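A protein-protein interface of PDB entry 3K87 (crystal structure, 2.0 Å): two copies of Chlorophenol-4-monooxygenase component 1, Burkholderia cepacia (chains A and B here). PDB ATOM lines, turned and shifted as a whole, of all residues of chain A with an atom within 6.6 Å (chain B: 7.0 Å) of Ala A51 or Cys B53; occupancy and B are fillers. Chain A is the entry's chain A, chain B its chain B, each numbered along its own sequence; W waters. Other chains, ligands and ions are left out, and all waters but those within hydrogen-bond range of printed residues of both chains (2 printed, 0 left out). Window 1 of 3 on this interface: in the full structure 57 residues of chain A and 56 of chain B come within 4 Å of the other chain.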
ATOM      1  N   LEU A  26     -15.868  -5.683 -16.194  1.00  0.00           N
ATOM      2  CA  LEU A  26     -15.829  -7.135 -15.978  1.00  0.00           C
ATOM      3  C   LEU A  26     -15.039  -7.809 -17.080  1.00  0.00           C
ATOM      4  O   LEU A  26     -14.440  -8.879 -16.850  1.00  0.00           O
ATOM      5  CB  LEU A  26     -17.213  -7.759 -15.906  1.00  0.00           C
ATOM      6  CG  LEU A  26     -18.028  -7.517 -14.637  1.00  0.00           C
ATOM      7  CD1 LEU A  26     -19.457  -8.113 -14.798  1.00  0.00           C
ATOM      8  CD2 LEU A  26     -17.273  -8.108 -13.438  1.00  0.00           C
ATOM      9  N   THR A  31     -12.216 -15.311 -16.016  1.00  0.00           N
ATOM     10  CA  THR A  31     -13.033 -16.357 -15.396  1.00  0.00           C
ATOM     11  C   THR A  31     -12.667 -17.678 -16.023  1.00  0.00           C
ATOM     12  O   THR A  31     -12.093 -17.699 -17.131  1.00  0.00           O
ATOM     13  CB  THR A  31     -14.552 -16.143 -15.699  1.00  0.00           C
ATOM     14  OG1 THR A  31     -14.806 -16.308 -17.111  1.00  0.00           O
ATOM     15  CG2 THR A  31     -15.019 -14.775 -15.289  1.00  0.00           C
ATOM     16  N   PRO A  32     -13.027 -18.795 -15.358  1.00  0.00           N
ATOM     17  CA  PRO A  32     -13.030 -20.060 -16.084  1.00  0.00           C
ATOM     18  C   PRO A  32     -14.200 -20.021 -17.046  1.00  0.00           C
ATOM     19  O   PRO A  32     -14.977 -19.054 -17.044  1.00  0.00           O
ATOM     20  CB  PRO A  32     -13.355 -21.092 -15.011  1.00  0.00           C
ATOM     21  CG  PRO A  32     -13.935 -20.342 -13.905  1.00  0.00           C
ATOM     22  CD  PRO A  32     -13.657 -18.901 -14.029  1.00  0.00           C
ATOM     23  N   THR A  34     -17.477 -22.635 -18.163  1.00  0.00           N
ATOM     24  CA  THR A  34     -18.060 -23.944 -17.958  1.00  0.00           C
ATOM     25  C   THR A  34     -19.201 -24.143 -18.926  1.00  0.00           C
ATOM     26  O   THR A  34     -19.676 -23.177 -19.510  1.00  0.00           O
ATOM     27  CB  THR A  34     -18.570 -24.169 -16.502  1.00  0.00           C
ATOM     28  OG1 THR A  34     -19.858 -23.557 -16.385  1.00  0.00           O
ATOM     29  CG2 THR A  34     -17.590 -23.558 -15.458  1.00  0.00           C
ATOM     30  N   CYS A  49     -21.481 -20.993 -19.189  1.00  0.00           N
ATOM     31  CA  CYS A  49     -21.602 -20.249 -17.953  1.00  0.00           C
ATOM     32  C   CYS A  49     -20.227 -20.049 -17.317  1.00  0.00           C
ATOM     33  O   CYS A  49     -19.470 -21.016 -17.095  1.00  0.00           O
ATOM     34  CB  CYS A  49     -22.585 -20.996 -16.983  1.00  0.00           C
ATOM     35  SG  CYS A  49     -22.753 -20.151 -15.379  1.00  0.00           S
ATOM     36  N   SER A  50     -19.886 -18.782 -17.068  1.00  0.00           N
ATOM     37  CA  SER A  50     -18.645 -18.429 -16.372  1.00  0.00           C
ATOM     38  C   SER A  50     -18.887 -17.966 -14.934  1.00  0.00           C
ATOM     39  O   SER A  50     -17.959 -17.941 -14.118  1.00  0.00           O
ATOM     40  CB  SER A  50     -17.917 -17.313 -17.131  1.00  0.00           C
ATOM     41  OG  SER A  50     -18.743 -16.149 -17.234  1.00  0.00           O
ATOM     42  N   ALA A  51     -20.114 -17.569 -14.617  1.00  0.00           N
ATOM     43  CA  ALA A  51     -20.433 -17.100 -13.256  1.00  0.00           C
ATOM     44  C   ALA A  51     -20.753 -18.267 -12.346  1.00  0.00           C
ATOM     45  O   ALA A  51     -21.923 -18.471 -11.980  1.00  0.00           O
ATOM     46  CB  ALA A  51     -21.609 -16.129 -13.301  1.00  0.00           C
ATOM     47  N   VAL A  52     -19.714 -19.015 -11.974  1.00  0.00           N
ATOM     48  CA  VAL A  52     -19.833 -20.231 -11.205  1.00  0.00           C
ATOM     49  C   VAL A  52     -18.764 -20.162 -10.116  1.00  0.00           C
ATOM     50  O   VAL A  52     -17.653 -19.696 -10.365  1.00  0.00           O
ATOM     51  CB  VAL A  52     -19.524 -21.484 -12.051  1.00  0.00           C
ATOM     52  CG1 VAL A  52     -19.557 -22.720 -11.173  1.00  0.00           C
ATOM     53  CG2 VAL A  52     -20.544 -21.704 -13.166  1.00  0.00           C
ATOM     54  N   CYS A  53     -19.069 -20.617  -8.909  1.00  0.00           N
ATOM     55  CA  CYS A  53     -17.984 -20.820  -7.952  1.00  0.00           C
ATOM     56  C   CYS A  53     -18.339 -21.776  -6.838  1.00  0.00           C
ATOM     57  O   CYS A  53     -19.512 -22.112  -6.599  1.00  0.00           O
ATOM     58  CB  CYS A  53     -17.498 -19.500  -7.346  1.00  0.00           C
ATOM     59  SG  CYS A  53     -18.759 -18.691  -6.329  1.00  0.00           S
ATOM     60  N   LEU A  63     -22.329 -22.778  -6.886  1.00  0.00           N
ATOM     61  CA  LEU A  63     -23.459 -21.976  -7.324  1.00  0.00           C
ATOM     62  C   LEU A  63     -23.145 -21.543  -8.732  1.00  0.00           C
ATOM     63  O   LEU A  63     -21.975 -21.437  -9.122  1.00  0.00           O
ATOM     64  CB  LEU A  63     -23.699 -20.786  -6.365  1.00  0.00           C
ATOM     65  CG  LEU A  63     -22.570 -19.749  -6.260  1.00  0.00           C
ATOM     66  CD1 LEU A  63     -22.400 -18.928  -7.569  1.00  0.00           C
ATOM     67  CD2 LEU A  63     -22.829 -18.804  -5.068  1.00  0.00           C
ATOM     68  N   LEU A  64     -24.194 -21.283  -9.491  1.00  0.00           N
ATOM     69  CA  LEU A  64     -24.058 -20.730 -10.817  1.00  0.00           C
ATOM     70  C   LEU A  64     -25.198 -19.701 -11.052  1.00  0.00           C
ATOM     71  O   LEU A  64     -26.313 -19.869 -10.580  1.00  0.00           O
ATOM     72  CB  LEU A  64     -24.063 -21.877 -11.859  1.00  0.00           C
ATOM     73  CG  LEU A  64     -25.274 -22.776 -11.803  1.00  0.00           C
ATOM     74  CD1 LEU A  64     -26.209 -22.406 -12.922  1.00  0.00           C
ATOM     75  CD2 LEU A  64     -24.854 -24.209 -11.912  1.00  0.00           C
ATOM     76  N   CYS A  65     -24.899 -18.618 -11.755  1.00  0.00           N
ATOM     77  CA  CYS A  65     -25.866 -17.548 -11.925  1.00  0.00           C
ATOM     78  C   CYS A  65     -26.226 -17.487 -13.386  1.00  0.00           C
ATOM     79  O   CYS A  65     -25.366 -17.263 -14.231  1.00  0.00           O
ATOM     80  CB  CYS A  65     -25.222 -16.224 -11.572  1.00  0.00           C
ATOM     81  SG  CYS A  65     -24.290 -16.277 -10.030  1.00  0.00           S
ATOM     82  N   ILE A  66     -27.494 -17.614 -13.685  1.00  0.00           N
ATOM     83  CA  ILE A  66     -27.906 -17.810 -15.059  1.00  0.00           C
ATOM     84  C   ILE A  66     -29.124 -16.927 -15.308  1.00  0.00           C
ATOM     85  O   ILE A  66     -29.999 -16.871 -14.472  1.00  0.00           O
ATOM     86  CB  ILE A  66     -28.148 -19.307 -15.225  1.00  0.00           C
ATOM     87  CG1 ILE A  66     -27.313 -19.834 -16.357  1.00  0.00           C
ATOM     88  CG2 ILE A  66     -29.576 -19.761 -15.078  1.00  0.00           C
ATOM     89  CD1 ILE A  66     -25.946 -20.012 -15.838  1.00  0.00           C
ATOM     90  N   HIS A 145     -30.956 -12.534 -12.938  1.00  0.00           N
ATOM     91  CA  HIS A 145     -30.354 -13.856 -12.821  1.00  0.00           C
ATOM     92  C   HIS A 145     -30.894 -14.706 -11.686  1.00  0.00           C
ATOM     93  O   HIS A 145     -31.121 -14.217 -10.581  1.00  0.00           O
ATOM     94  CB  HIS A 145     -28.833 -13.733 -12.657  1.00  0.00           C
ATOM     95  CG  HIS A 145     -28.118 -13.511 -13.949  1.00  0.00           C
ATOM     96  ND1 HIS A 145     -28.424 -12.457 -14.788  1.00  0.00           N
ATOM     97  CD2 HIS A 145     -27.130 -14.207 -14.554  1.00  0.00           C
ATOM     98  CE1 HIS A 145     -27.628 -12.489 -15.839  1.00  0.00           C
ATOM     99  NE2 HIS A 145     -26.837 -13.548 -15.729  1.00  0.00           N
ATOM    100  N   SER B  50     -11.097 -16.523  -4.036  1.00  0.00           N
ATOM    101  CA  SER B  50     -11.301 -16.823  -5.460  1.00  0.00           C
ATOM    102  C   SER B  50     -12.738 -17.153  -5.765  1.00  0.00           C
ATOM    103  O   SER B  50     -13.078 -17.313  -6.926  1.00  0.00           O
ATOM    104  CB  SER B  50     -10.451 -18.022  -5.902  1.00  0.00           C
ATOM    105  OG  SER B  50     -10.632 -19.078  -4.961  1.00  0.00           O
ATOM    106  N   ALA B  51     -13.569 -17.285  -4.735  1.00  0.00           N
ATOM    107  CA  ALA B  51     -14.928 -17.751  -4.930  1.00  0.00           C
ATOM    108  C   ALA B  51     -15.777 -16.498  -5.076  1.00  0.00           C
ATOM    109  O   ALA B  51     -16.465 -16.052  -4.120  1.00  0.00           O
ATOM    110  CB  ALA B  51     -15.387 -18.641  -3.744  1.00  0.00           C
ATOM    111  N   VAL B  52     -15.730 -15.943  -6.291  1.00  0.00           N
ATOM    112  CA  VAL B  52     -16.320 -14.641  -6.615  1.00  0.00           C
ATOM    113  C   VAL B  52     -16.888 -14.747  -8.004  1.00  0.00           C
ATOM    114  O   VAL B  52     -16.283 -15.385  -8.876  1.00  0.00           O
ATOM    115  CB  VAL B  52     -15.224 -13.574  -6.687  1.00  0.00           C
ATOM    116  CG1 VAL B  52     -15.766 -12.312  -7.235  1.00  0.00           C
ATOM    117  CG2 VAL B  52     -14.632 -13.374  -5.347  1.00  0.00           C
ATOM    118  N   CYS B  53     -18.044 -14.139  -8.234  1.00  0.00           N
ATOM    119  CA  CYS B  53     -18.484 -13.954  -9.601  1.00  0.00           C
ATOM    120  C   CYS B  53     -19.469 -12.825  -9.756  1.00  0.00           C
ATOM    121  O   CYS B  53     -20.012 -12.308  -8.762  1.00  0.00           O
ATOM    122  CB  CYS B  53     -19.067 -15.256 -10.170  1.00  0.00           C
ATOM    123  SG  CYS B  53     -20.534 -15.764  -9.323  1.00  0.00           S
ATOM    124  N   SER B  54     -19.708 -12.434 -11.003  1.00  0.00           N
ATOM    125  CA  SER B  54     -20.653 -11.349 -11.254  1.00  0.00           C
ATOM    126  C   SER B  54     -22.008 -11.984 -11.287  1.00  0.00           C
ATOM    127  O   SER B  54     -22.140 -13.139 -11.679  1.00  0.00           O
ATOM    128  CB  SER B  54     -20.381 -10.593 -12.569  1.00  0.00           C
ATOM    129  OG  SER B  54     -20.164 -11.492 -13.638  1.00  0.00           O
ATOM    130  N   VAL B  55     -23.017 -11.235 -10.876  1.00  0.00           N
ATOM    131  CA  VAL B  55     -24.342 -11.818 -10.699  1.00  0.00           C
ATOM    132  C   VAL B  55     -25.333 -11.252 -11.719  1.00  0.00           C
ATOM    133  O   VAL B  55     -25.920 -12.012 -12.476  1.00  0.00           O
ATOM    134  CB  VAL B  55     -24.844 -11.620  -9.269  1.00  0.00           C
ATOM    135  CG1 VAL B  55     -26.355 -12.071  -9.127  1.00  0.00           C
ATOM    136  CG2 VAL B  55     -23.919 -12.376  -8.250  1.00  0.00           C
ATOM    137  N   CYS B  56     -25.529  -9.932 -11.733  1.00  0.00           N
ATOM    138  CA  CYS B  56     -26.355  -9.314 -12.741  1.00  0.00           C
ATOM    139  C   CYS B  56     -25.842  -7.896 -12.904  1.00  0.00           C
ATOM    140  O   CYS B  56     -25.052  -7.413 -12.094  1.00  0.00           O
ATOM    141  CB  CYS B  56     -27.831  -9.271 -12.318  1.00  0.00           C
ATOM    142  SG  CYS B  56     -28.060  -8.514 -10.673  1.00  0.00           S
ATOM    143  N   THR B  61     -24.179  -6.222  -9.439  1.00  0.00           N
ATOM    144  CA  THR B  61     -23.986  -7.021  -8.233  1.00  0.00           C
ATOM    145  C   THR B  61     -22.941  -8.086  -8.499  1.00  0.00           C
ATOM    146  O   THR B  61     -22.951  -8.731  -9.577  1.00  0.00           O
ATOM    147  CB  THR B  61     -25.271  -7.746  -7.868  1.00  0.00           C
ATOM    148  OG1 THR B  61     -26.326  -6.785  -7.803  1.00  0.00           O
ATOM    149  CG2 THR B  61     -25.127  -8.536  -6.523  1.00  0.00           C
ATOM    150  N   VAL B  62     -22.047  -8.255  -7.532  1.00  0.00           N
ATOM    151  CA  VAL B  62     -21.127  -9.395  -7.506  1.00  0.00           C
ATOM    152  C   VAL B  62     -21.422 -10.199  -6.223  1.00  0.00           C
ATOM    153  O   VAL B  62     -22.138  -9.712  -5.342  1.00  0.00           O
ATOM    154  CB  VAL B  62     -19.661  -8.912  -7.539  1.00  0.00           C
ATOM    155  CG1 VAL B  62     -19.407  -8.079  -8.800  1.00  0.00           C
ATOM    156  CG2 VAL B  62     -19.310  -8.131  -6.218  1.00  0.00           C
ATOM    157  N   LEU B  63     -20.959 -11.445  -6.143  1.00  0.00           N
ATOM    158  CA  LEU B  63     -21.051 -12.203  -4.913  1.00  0.00           C
ATOM    159  C   LEU B  63     -19.664 -12.775  -4.600  1.00  0.00           C
ATOM    160  O   LEU B  63     -18.796 -12.858  -5.471  1.00  0.00           O
ATOM    161  CB  LEU B  63     -22.116 -13.296  -4.967  1.00  0.00           C
ATOM    162  CG  LEU B  63     -21.874 -14.507  -5.892  1.00  0.00           C
ATOM    163  CD1 LEU B  63     -20.805 -15.473  -5.354  1.00  0.00           C
ATOM    164  CD2 LEU B  63     -23.201 -15.225  -6.078  1.00  0.00           C
ATOM    165  N   LEU B  64     -19.454 -13.113  -3.342  1.00  0.00           N
ATOM    166  CA  LEU B  64     -18.220 -13.701  -2.893  1.00  0.00           C
ATOM    167  C   LEU B  64     -18.555 -14.610  -1.714  1.00  0.00           C
ATOM    168  O   LEU B  64     -19.460 -14.319  -0.920  1.00  0.00           O
ATOM    169  CB  LEU B  64     -17.246 -12.601  -2.489  1.00  0.00           C
ATOM    170  CG  LEU B  64     -17.841 -11.563  -1.568  1.00  0.00           C
ATOM    171  CD1 LEU B  64     -17.070 -11.692  -0.335  1.00  0.00           C
ATOM    172  CD2 LEU B  64     -17.617 -10.201  -2.204  1.00  0.00           C
ATOM    173  N   CYS B  65     -17.839 -15.717  -1.634  1.00  0.00           N
ATOM    174  CA  CYS B  65     -18.084 -16.748  -0.637  1.00  0.00           C
ATOM    175  C   CYS B  65     -16.915 -16.830   0.264  1.00  0.00           C
ATOM    176  O   CYS B  65     -15.807 -17.216  -0.164  1.00  0.00           O
ATOM    177  CB  CYS B  65     -18.271 -18.103  -1.308  1.00  0.00           C
ATOM    178  SG  CYS B  65     -19.655 -18.004  -2.458  1.00  0.00           S
ATOM    179  N   TRP B  86      -9.425  -7.841  -8.283  1.00  0.00           N
ATOM    180  CA  TRP B  86      -8.884  -8.901  -9.133  1.00  0.00           C
ATOM    181  C   TRP B  86      -7.385  -8.619  -9.361  1.00  0.00           C
ATOM    182  O   TRP B  86      -7.017  -7.562  -9.895  1.00  0.00           O
ATOM    183  CB  TRP B  86      -9.653  -8.881 -10.472  1.00  0.00           C
ATOM    184  CG  TRP B  86     -11.010  -9.582 -10.491  1.00  0.00           C
ATOM    185  CD1 TRP B  86     -11.264 -10.869 -10.907  1.00  0.00           C
ATOM    186  CD2 TRP B  86     -12.275  -9.026 -10.105  1.00  0.00           C
ATOM    187  NE1 TRP B  86     -12.616 -11.146 -10.806  1.00  0.00           N
ATOM    188  CE2 TRP B  86     -13.261 -10.035 -10.326  1.00  0.00           C
ATOM    189  CE3 TRP B  86     -12.684  -7.763  -9.626  1.00  0.00           C
ATOM    190  CZ2 TRP B  86     -14.631  -9.834 -10.054  1.00  0.00           C
ATOM    191  CZ3 TRP B  86     -14.069  -7.554  -9.353  1.00  0.00           C
ATOM    192  CH2 TRP B  86     -15.011  -8.598  -9.558  1.00  0.00           C
HETATM  193  O   HOH W   1     -19.366 -14.097 -15.530  1.00  0.00           O
HETATM  194  O   HOH W   2     -23.946 -13.428 -13.779  1.00  0.00           O
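A ring nitrogen (ND1) of His A145 lies close to the backbone carbonyl oxygen (O) of Val B55, 3.4 Å away.
O of Cys B53 is in hydrogen-bond range of N of Leu B63, 2.9 Å away.
O of Ala A51 lies within hydrogen-bond range of N of Cys A65.
N of Val B55 sits at hydrogen-bond distance from O of Thr B61.
The side-chain sulfur (SG) of Cys A49 lies close to the backbone NH (N) of Ala A51.
The backbone carbonyl oxygen (O) of Ala B51 sits at hydrogen-bond distance from the backbone NH (N) of Cys B65, at 2.9 Å.
O of Cys A53 sits at hydrogen-bond distance from N of Leu A63, at 2.9 Å.
Among the printed residues, merely in contact across the chains: Ala A51 with Ser B54, Leu A26 with Ser B54, Leu A63 with Leu B63, Ala A51 with Cys B53, Cys A65 with Cys B53, Cys A53 with Ala B51 and Cys A53 with Leu B63.
Ala A51 touches just these residues of chain B: Cys B53 (3.8 Å) and Ser B54 (3.4 Å).
Cys B53 touches two residues of chain A.
Of the printed residues of chain A, Leu B63 touches Cys A53 (3.9 Å) and Leu A63 (3.7 Å).
Of the printed residues of chain A, Ala B51 touches Cys A53.
Of the printed residues of chain B, Leu A63 touches Leu B63.
Of the printed residues of chain A, Ser B54 touches Leu A26 and Ala A51.
Of the printed residues of chain B, Leu A26 touches Ser B54.
Trp B86 touches none of the printed residues of chain A.
Cys B65 touches none of the printed residues of chain A.
The nearest residue of chain A that does not touch Cys B53 is Leu A63 (4.1 Å).
Of the 14 printed residues of chain A, 6 touch a printed residue of chain B.
Hydrophobic or aromatic side chains of chain A that line the printed part of chain B: Leu A26, Ala A51, Leu A63 and His A145.
Along chain A the printed residues that touch a printed residue of chain B span positions 26 to 145.
Of the 13 printed residues of chain B, 5 touch a printed residue of chain A.
Hydrophobic or aromatic side chains of chain B that line the printed part of chain A: Leu B63.
Ala A51 touches Cys B53, and with the chains exchanged Cys A53 touches Ala B51.
Cys A53 touches Leu B63, but with the chains exchanged Leu A63 does not touch Cys B53 (4.1 Å).
Leu A63 touches its own counterpart, Leu B63.
Cys A65 touches Cys B53, but with the chains exchanged Cys A53 does not touch Cys B65 (4.03 Å).
Of the 8 pairs that touch across the chains among the printed residues, 3 have their exchanged pair printed and touching as well.
Water W1 lies within hydrogen-bond range of OG of Ser A50 (2.7 Å) and OG of Ser B54 (3.3 Å).
Water W2 lies within hydrogen-bond range of O of Val B55 (2.8 Å), O of Ser B54 (2.8 Å) and NE2 of His A145 (3.5 Å).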
